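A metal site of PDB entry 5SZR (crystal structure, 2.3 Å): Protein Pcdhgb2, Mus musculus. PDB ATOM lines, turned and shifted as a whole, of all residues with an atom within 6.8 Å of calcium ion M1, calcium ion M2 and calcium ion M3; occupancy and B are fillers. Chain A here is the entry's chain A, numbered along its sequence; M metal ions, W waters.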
ATOM      1  N   GLU A 121       7.662  -3.189 -30.846  1.00  0.00           N
ATOM      2  CA  GLU A 121       7.393  -2.246 -29.763  1.00  0.00           C
ATOM      3  C   GLU A 121       8.021  -0.876 -29.986  1.00  0.00           C
ATOM      4  O   GLU A 121       7.638   0.082 -29.319  1.00  0.00           O
ATOM      5  CB  GLU A 121       7.896  -2.827 -28.437  1.00  0.00           C
ATOM      6  CG  GLU A 121       9.409  -2.905 -28.327  1.00  0.00           C
ATOM      7  CD  GLU A 121       9.851  -3.419 -26.982  1.00  0.00           C
ATOM      8  OE1 GLU A 121      10.792  -4.240 -26.940  1.00  0.00           O
ATOM      9  OE2 GLU A 121       9.254  -3.026 -25.959  1.00  0.00           O
ATOM     10  N   LEU A 173       4.828   2.263 -27.920  1.00  0.00           N
ATOM     11  CA  LEU A 173       4.513   0.957 -27.377  1.00  0.00           C
ATOM     12  C   LEU A 173       5.623   0.489 -26.439  1.00  0.00           C
ATOM     13  O   LEU A 173       6.717   1.066 -26.386  1.00  0.00           O
ATOM     14  CB  LEU A 173       4.304  -0.042 -28.507  1.00  0.00           C
ATOM     15  CG  LEU A 173       3.163   0.362 -29.466  1.00  0.00           C
ATOM     16  CD1 LEU A 173       3.288  -0.359 -30.799  1.00  0.00           C
ATOM     17  CD2 LEU A 173       1.812   0.085 -28.833  1.00  0.00           C
ATOM     18  N   ASP A 174       5.329  -0.565 -25.674  1.00  0.00           N
ATOM     19  CA  ASP A 174       6.304  -1.117 -24.743  1.00  0.00           C
ATOM     20  C   ASP A 174       5.882  -2.546 -24.435  1.00  0.00           C
ATOM     21  O   ASP A 174       4.937  -2.766 -23.682  1.00  0.00           O
ATOM     22  CB  ASP A 174       6.396  -0.272 -23.469  1.00  0.00           C
ATOM     23  CG  ASP A 174       7.404  -0.826 -22.470  1.00  0.00           C
ATOM     24  OD1 ASP A 174       8.223  -1.686 -22.854  1.00  0.00           O
ATOM     25  OD2 ASP A 174       7.386  -0.388 -21.307  1.00  0.00           O
ATOM     26  N   ARG A 175       6.607  -3.518 -25.006  1.00  0.00           N
ATOM     27  CA  ARG A 175       6.285  -4.922 -24.787  1.00  0.00           C
ATOM     28  C   ARG A 175       6.386  -5.278 -23.311  1.00  0.00           C
ATOM     29  O   ARG A 175       5.579  -6.079 -22.810  1.00  0.00           O
ATOM     30  CB  ARG A 175       7.212  -5.816 -25.614  1.00  0.00           C
ATOM     31  CG  ARG A 175       6.785  -7.267 -25.617  1.00  0.00           C
ATOM     32  CD  ARG A 175       7.939  -8.191 -25.942  1.00  0.00           C
ATOM     33  NE  ARG A 175       8.926  -8.230 -24.858  1.00  0.00           N
ATOM     34  CZ  ARG A 175       8.836  -9.029 -23.797  1.00  0.00           C
ATOM     35  NH1 ARG A 175       7.809  -9.849 -23.683  1.00  0.00           N
ATOM     36  NH2 ARG A 175       9.768  -8.998 -22.859  1.00  0.00           N
ATOM     37  N   GLU A 176       7.367  -4.715 -22.611  1.00  0.00           N
ATOM     38  CA  GLU A 176       7.555  -5.047 -21.199  1.00  0.00           C
ATOM     39  C   GLU A 176       6.379  -4.616 -20.336  1.00  0.00           C
ATOM     40  O   GLU A 176       6.201  -5.156 -19.242  1.00  0.00           O
ATOM     41  CB  GLU A 176       8.863  -4.431 -20.696  1.00  0.00           C
ATOM     42  CG  GLU A 176      10.127  -5.211 -21.090  1.00  0.00           C
ATOM     43  CD  GLU A 176      10.487  -5.079 -22.563  1.00  0.00           C
ATOM     44  OE1 GLU A 176      10.393  -3.952 -23.106  1.00  0.00           O
ATOM     45  OE2 GLU A 176      10.863  -6.095 -23.181  1.00  0.00           O
ATOM     46  N   ALA A 177       5.567  -3.662 -20.798  1.00  0.00           N
ATOM     47  CA  ALA A 177       4.377  -3.226 -20.081  1.00  0.00           C
ATOM     48  C   ALA A 177       3.106  -3.901 -20.575  1.00  0.00           C
ATOM     49  O   ALA A 177       2.328  -4.423 -19.766  1.00  0.00           O
ATOM     50  CB  ALA A 177       4.236  -1.702 -20.156  1.00  0.00           C
ATOM     51  N   SER A 206       6.146  -7.417 -30.541  1.00  0.00           N
ATOM     52  CA  SER A 206       7.412  -8.143 -30.558  1.00  0.00           C
ATOM     53  C   SER A 206       8.497  -7.348 -29.827  1.00  0.00           C
ATOM     54  O   SER A 206       8.413  -6.130 -29.658  1.00  0.00           O
ATOM     55  CB  SER A 206       7.852  -8.424 -31.998  1.00  0.00           C
ATOM     56  OG  SER A 206       7.983  -7.234 -32.738  1.00  0.00           O
ATOM     57  N   ASP A 207       9.528  -8.061 -29.391  1.00  0.00           N
ATOM     58  CA  ASP A 207      10.525  -7.499 -28.481  1.00  0.00           C
ATOM     59  C   ASP A 207      11.647  -6.802 -29.236  1.00  0.00           C
ATOM     60  O   ASP A 207      12.045  -7.219 -30.336  1.00  0.00           O
ATOM     61  CB  ASP A 207      11.117  -8.586 -27.583  1.00  0.00           C
ATOM     62  CG  ASP A 207      12.114  -8.033 -26.568  1.00  0.00           C
ATOM     63  OD1 ASP A 207      11.705  -7.209 -25.721  1.00  0.00           O
ATOM     64  OD2 ASP A 207      13.291  -8.441 -26.605  1.00  0.00           O
ATOM     65  N   VAL A 208      12.155  -5.727 -28.632  1.00  0.00           N
ATOM     66  CA  VAL A 208      13.353  -5.018 -29.063  1.00  0.00           C
ATOM     67  C   VAL A 208      14.288  -4.966 -27.856  1.00  0.00           C
ATOM     68  O   VAL A 208      13.840  -4.978 -26.705  1.00  0.00           O
ATOM     69  CB  VAL A 208      13.009  -3.602 -29.579  1.00  0.00           C
ATOM     70  CG1 VAL A 208      14.250  -2.760 -29.800  1.00  0.00           C
ATOM     71  CG2 VAL A 208      12.212  -3.708 -30.876  1.00  0.00           C
ATOM     72  N   ASN A 209      15.600  -4.968 -28.117  1.00  0.00           N
ATOM     73  CA  ASN A 209      16.585  -4.904 -27.043  1.00  0.00           C
ATOM     74  C   ASN A 209      16.684  -3.455 -26.574  1.00  0.00           C
ATOM     75  O   ASN A 209      17.597  -2.702 -26.947  1.00  0.00           O
ATOM     76  CB  ASN A 209      17.936  -5.435 -27.494  1.00  0.00           C
ATOM     77  CG  ASN A 209      18.926  -5.558 -26.349  1.00  0.00           C
ATOM     78  OD1 ASN A 209      18.529  -5.705 -25.188  1.00  0.00           O
ATOM     79  ND2 ASN A 209      20.209  -5.509 -26.663  1.00  0.00           N
ATOM     80  N   ASP A 210      15.739  -3.056 -25.724  1.00  0.00           N
ATOM     81  CA  ASP A 210      15.733  -1.704 -25.173  1.00  0.00           C
ATOM     82  C   ASP A 210      15.900  -1.686 -23.653  1.00  0.00           C
ATOM     83  O   ASP A 210      15.609  -0.673 -23.021  1.00  0.00           O
ATOM     84  CB  ASP A 210      14.452  -0.964 -25.582  1.00  0.00           C
ATOM     85  CG  ASP A 210      13.185  -1.742 -25.234  1.00  0.00           C
ATOM     86  OD1 ASP A 210      13.274  -2.973 -25.022  1.00  0.00           O
ATOM     87  OD2 ASP A 210      12.101  -1.119 -25.196  1.00  0.00           O
ATOM     88  N   ASN A 211      16.370  -2.781 -23.056  1.00  0.00           N
ATOM     89  CA  ASN A 211      16.590  -2.855 -21.617  1.00  0.00           C
ATOM     90  C   ASN A 211      17.991  -3.362 -21.338  1.00  0.00           C
ATOM     91  O   ASN A 211      18.356  -4.451 -21.773  1.00  0.00           O
ATOM     92  CB  ASN A 211      15.557  -3.759 -20.940  1.00  0.00           C
ATOM     93  CG  ASN A 211      14.172  -3.138 -20.905  1.00  0.00           C
ATOM     94  OD1 ASN A 211      13.866  -2.342 -20.004  1.00  0.00           O
ATOM     95  ND2 ASN A 211      13.339  -3.497 -21.866  1.00  0.00           N
ATOM     96  N   ALA A 212      18.766  -2.568 -20.614  1.00  0.00           N
ATOM     97  CA  ALA A 212      20.102  -2.990 -20.211  1.00  0.00           C
ATOM     98  C   ALA A 212      20.013  -3.896 -18.987  1.00  0.00           C
ATOM     99  O   ALA A 212      19.128  -3.698 -18.134  1.00  0.00           O
ATOM    100  CB  ALA A 212      20.976  -1.774 -19.899  1.00  0.00           C
ATOM    101  N   PRO A 213      20.868  -4.902 -18.876  1.00  0.00           N
ATOM    102  CA  PRO A 213      20.912  -5.701 -17.652  1.00  0.00           C
ATOM    103  C   PRO A 213      21.156  -4.825 -16.431  1.00  0.00           C
ATOM    104  O   PRO A 213      21.806  -3.781 -16.510  1.00  0.00           O
ATOM    105  CB  PRO A 213      22.074  -6.677 -17.888  1.00  0.00           C
ATOM    106  CG  PRO A 213      22.815  -6.137 -19.079  1.00  0.00           C
ATOM    107  CD  PRO A 213      21.806  -5.402 -19.897  1.00  0.00           C
ATOM    108  N   ASP A 241      17.235  -8.894 -16.797  1.00  0.00           N
ATOM    109  CA  ASP A 241      16.995  -8.245 -18.080  1.00  0.00           C
ATOM    110  C   ASP A 241      15.625  -8.657 -18.603  1.00  0.00           C
ATOM    111  O   ASP A 241      15.428  -9.829 -18.963  1.00  0.00           O
ATOM    112  CB  ASP A 241      18.100  -8.621 -19.066  1.00  0.00           C
ATOM    113  CG  ASP A 241      18.101  -7.766 -20.326  1.00  0.00           C
ATOM    114  OD1 ASP A 241      17.047  -7.620 -20.964  1.00  0.00           O
ATOM    115  OD2 ASP A 241      19.176  -7.243 -20.683  1.00  0.00           O
ATOM    116  N   PRO A 242      14.647  -7.740 -18.658  1.00  0.00           N
ATOM    117  CA  PRO A 242      13.274  -8.145 -18.997  1.00  0.00           C
ATOM    118  C   PRO A 242      13.058  -8.454 -20.465  1.00  0.00           C
ATOM    119  O   PRO A 242      11.983  -8.948 -20.818  1.00  0.00           O
ATOM    120  CB  PRO A 242      12.452  -6.926 -18.577  1.00  0.00           C
ATOM    121  CG  PRO A 242      13.362  -5.784 -18.790  1.00  0.00           C
ATOM    122  CD  PRO A 242      14.751  -6.290 -18.420  1.00  0.00           C
ATOM    123  N   ASP A 243      14.037  -8.193 -21.327  1.00  0.00           N
ATOM    124  CA  ASP A 243      13.881  -8.455 -22.752  1.00  0.00           C
ATOM    125  C   ASP A 243      13.822  -9.966 -23.018  1.00  0.00           C
ATOM    126  O   ASP A 243      14.074 -10.791 -22.135  1.00  0.00           O
ATOM    127  CB  ASP A 243      15.014  -7.790 -23.543  1.00  0.00           C
ATOM    128  CG  ASP A 243      15.031  -6.277 -23.372  1.00  0.00           C
ATOM    129  OD1 ASP A 243      13.953  -5.687 -23.140  1.00  0.00           O
ATOM    130  OD2 ASP A 243      16.117  -5.675 -23.468  1.00  0.00           O
ATOM    131  N   LEU A 244      13.497 -10.321 -24.259  1.00  0.00           N
ATOM    132  CA  LEU A 244      13.219 -11.704 -24.619  1.00  0.00           C
ATOM    133  C   LEU A 244      14.396 -12.346 -25.350  1.00  0.00           C
ATOM    134  O   LEU A 244      15.128 -11.696 -26.095  1.00  0.00           O
ATOM    135  CB  LEU A 244      11.979 -11.795 -25.511  1.00  0.00           C
ATOM    136  CG  LEU A 244      10.601 -11.774 -24.850  1.00  0.00           C
ATOM    137  CD1 LEU A 244       9.524 -11.977 -25.910  1.00  0.00           C
ATOM    138  CD2 LEU A 244      10.505 -12.818 -23.751  1.00  0.00           C
ATOM    139  N   SER A 246      17.544 -13.712 -26.948  1.00  0.00           N
ATOM    140  CA  SER A 246      18.910 -13.210 -27.010  1.00  0.00           C
ATOM    141  C   SER A 246      19.039 -11.828 -26.391  1.00  0.00           C
ATOM    142  O   SER A 246      20.102 -11.483 -25.870  1.00  0.00           O
ATOM    143  CB  SER A 246      19.402 -13.187 -28.458  1.00  0.00           C
ATOM    144  OG  SER A 246      19.945 -14.442 -28.831  1.00  0.00           O
ATOM    145  N   ASN A 247      17.975 -11.022 -26.428  1.00  0.00           N
ATOM    146  CA  ASN A 247      18.033  -9.695 -25.835  1.00  0.00           C
ATOM    147  C   ASN A 247      18.059  -9.725 -24.314  1.00  0.00           C
ATOM    148  O   ASN A 247      18.353  -8.702 -23.685  1.00  0.00           O
ATOM    149  CB  ASN A 247      16.849  -8.860 -26.314  1.00  0.00           C
ATOM    150  CG  ASN A 247      16.818  -8.693 -27.821  1.00  0.00           C
ATOM    151  OD1 ASN A 247      17.833  -8.835 -28.494  1.00  0.00           O
ATOM    152  ND2 ASN A 247      15.644  -8.397 -28.353  1.00  0.00           N
ATOM    153  N   GLY A 248      17.748 -10.869 -23.694  1.00  0.00           N
ATOM    154  CA  GLY A 248      17.762 -10.977 -22.257  1.00  0.00           C
ATOM    155  C   GLY A 248      18.710 -12.025 -21.727  1.00  0.00           C
ATOM    156  O   GLY A 248      18.676 -12.374 -20.542  1.00  0.00           O
ATOM    157  N   LEU A 249      19.584 -12.539 -22.590  1.00  0.00           N
ATOM    158  CA  LEU A 249      20.588 -13.531 -22.203  1.00  0.00           C
ATOM    159  C   LEU A 249      21.828 -12.792 -21.705  1.00  0.00           C
ATOM    160  O   LEU A 249      22.418 -12.001 -22.438  1.00  0.00           O
ATOM    161  CB  LEU A 249      20.931 -14.434 -23.381  1.00  0.00           C
ATOM    162  CG  LEU A 249      21.859 -15.619 -23.104  1.00  0.00           C
ATOM    163  CD1 LEU A 249      21.234 -16.572 -22.102  1.00  0.00           C
ATOM    164  CD2 LEU A 249      22.214 -16.347 -24.393  1.00  0.00           C
ATOM    165  N   ILE A 250      22.234 -13.079 -20.462  1.00  0.00           N
ATOM    166  CA  ILE A 250      23.288 -12.328 -19.783  1.00  0.00           C
ATOM    167  C   ILE A 250      24.599 -13.096 -19.819  1.00  0.00           C
ATOM    168  O   ILE A 250      24.632 -14.320 -19.629  1.00  0.00           O
ATOM    169  CB  ILE A 250      22.901 -12.024 -18.321  1.00  0.00           C
ATOM    170  CG1 ILE A 250      21.518 -11.366 -18.250  1.00  0.00           C
ATOM    171  CG2 ILE A 250      23.937 -11.128 -17.666  1.00  0.00           C
ATOM    172  CD1 ILE A 250      21.467 -10.047 -18.951  1.00  0.00           C
ATOM    173  N   ASP A 299      24.100  -8.152 -22.307  1.00  0.00           N
ATOM    174  CA  ASP A 299      23.121  -8.980 -22.991  1.00  0.00           C
ATOM    175  C   ASP A 299      23.617  -9.329 -24.396  1.00  0.00           C
ATOM    176  O   ASP A 299      24.640  -8.821 -24.862  1.00  0.00           O
ATOM    177  CB  ASP A 299      21.733  -8.320 -23.019  1.00  0.00           C
ATOM    178  CG  ASP A 299      21.666  -7.056 -23.895  1.00  0.00           C
ATOM    179  OD1 ASP A 299      22.370  -6.946 -24.907  1.00  0.00           O
ATOM    180  OD2 ASP A 299      20.860  -6.172 -23.543  1.00  0.00           O
ATOM    181  N   HIS A 300      22.885 -10.212 -25.070  1.00  0.00           N
ATOM    182  CA  HIS A 300      23.250 -10.686 -26.402  1.00  0.00           C
ATOM    183  C   HIS A 300      22.298 -10.152 -27.475  1.00  0.00           C
ATOM    184  O   HIS A 300      21.892 -10.883 -28.381  1.00  0.00           O
ATOM    185  CB  HIS A 300      23.309 -12.207 -26.435  1.00  0.00           C
ATOM    186  CG  HIS A 300      24.440 -12.790 -25.662  1.00  0.00           C
ATOM    187  ND1 HIS A 300      25.748 -12.718 -26.098  1.00  0.00           N
ATOM    188  CD2 HIS A 300      24.474 -13.443 -24.475  1.00  0.00           C
ATOM    189  CE1 HIS A 300      26.541 -13.315 -25.219  1.00  0.00           C
ATOM    190  NE2 HIS A 300      25.794 -13.756 -24.227  1.00  0.00           N
ATOM    191  N   GLY A 301      21.944  -8.865 -27.376  1.00  0.00           N
ATOM    192  CA  GLY A 301      21.125  -8.215 -28.378  1.00  0.00           C
ATOM    193  C   GLY A 301      21.959  -7.418 -29.372  1.00  0.00           C
ATOM    194  O   GLY A 301      23.173  -7.300 -29.276  1.00  0.00           O
ATOM    195  N   LEU A 305      23.555  -4.331 -24.731  1.00  0.00           N
ATOM    196  CA  LEU A 305      23.453  -3.429 -23.591  1.00  0.00           C
ATOM    197  C   LEU A 305      24.167  -4.062 -22.404  1.00  0.00           C
ATOM    198  O   LEU A 305      24.302  -5.288 -22.320  1.00  0.00           O
ATOM    199  CB  LEU A 305      21.989  -3.133 -23.265  1.00  0.00           C
ATOM    200  CG  LEU A 305      21.299  -2.330 -24.364  1.00  0.00           C
ATOM    201  CD1 LEU A 305      19.793  -2.274 -24.125  1.00  0.00           C
ATOM    202  CD2 LEU A 305      21.878  -0.932 -24.435  1.00  0.00           C
HETATM  203 CA    CA M   1      10.221  -1.849 -24.057  1.00  0.00          CA
HETATM  204 CA    CA M   2      12.275  -5.103 -24.905  1.00  0.00          CA
HETATM  205 CA    CA M   3      18.331  -6.492 -22.926  1.00  0.00          CA
HETATM  206  O   HOH W   1      11.290  -1.025 -21.937  1.00  0.00           O
HETATM  207  O   HOH W   2       9.440   0.361 -24.527  1.00  0.00           O
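N of Leu 244 lies within hydrogen-bond range of OD2 of Asp 207, at 3.0 Å. The side-chain carboxylate (OD1) of Asp 299 sits at hydrogen-bond distance from the backbone NH (N) of Gly 301 (3.2 Å). The side-chain carboxylate (OE2) of Glu 176 sits close to the guanidinium group (NH2) of Arg 175, 3.1 Å away. OD2 of Asp 207 sits at hydrogen-bond distance from ND2 of Asn 247 (2.9 Å). The backbone NH (N) of Glu 121 is in hydrogen-bond range of the backbone carbonyl oxygen (O) of Ser 206. The side-chain carboxylate (OD1) of Asp 210 lies close to the side-chain amide nitrogen (ND2) of Asn 211 (3.2 Å). N of Asp 299 is in hydrogen-bond range of O of Leu 305 (2.9 Å). ND2 of Asn 211 lies close to OE1 of Glu 176, 3.2 Å away.
Within 4 Å of calcium ion M1: Glu 121, Asp 174, Glu 176 and Asp 210.
Of the 27 residues printed, 7 come within 4 Å of calcium ion M2. The nearest printed residue that does not touch calcium ion M2 is Arg 175 (4.6 Å).
Within 4 Å of calcium ion M3: Asn 209, Asn 211, Asp 241, Asp 243, Asn 247 and Asp 299.
Calcium ion M1 is bound by the side-chain carboxylate of Glu 176 (2.3 Å), the side-chain carboxylate of Asp 210 (2.3 Å), the side-chain carboxylate of Asp 174 (2.3 Å), water W2 (2.4 Å), the side-chain carboxylate of Glu 121 (2.4 Å) and water W1 (2.5 Å). Calcium ion M1 has six donor atoms within binding distance.
Calcium ion M2 is bound by OD1 of Asp 207 (2.3 Å), OD1 of Asp 210 (2.4 Å), O of Val 208 (2.4 Å), OE2 of Glu 176 (2.4 Å), OD1 of Asp 243 (2.5 Å), OE1 of Glu 121 (2.7 Å) and OE1 of Glu 176 (2.8 Å).
The backbone carbonyl oxygen (O) of Asn 247 is bound to calcium ion M3 (2.3 Å). Calcium ion M3 is bound by the backbone carbonyl oxygen (O) of Asn 211 (2.3 Å). Calcium ion M3 is bound by the side-chain amide oxygen (OD1) of Asn 209 (2.4 Å). The side-chain carboxylate (OD2) of Asp 243 binds calcium ion M3, 2.4 Å away. Calcium ion M3 is bound by OD2 of Asp 241 (2.5 Å). OD1 of Asp 241 is bound to calcium ion M3 (2.6 Å). The side-chain carboxylate (OD2) of Asp 299 binds calcium ion M3, 2.6 Å away.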
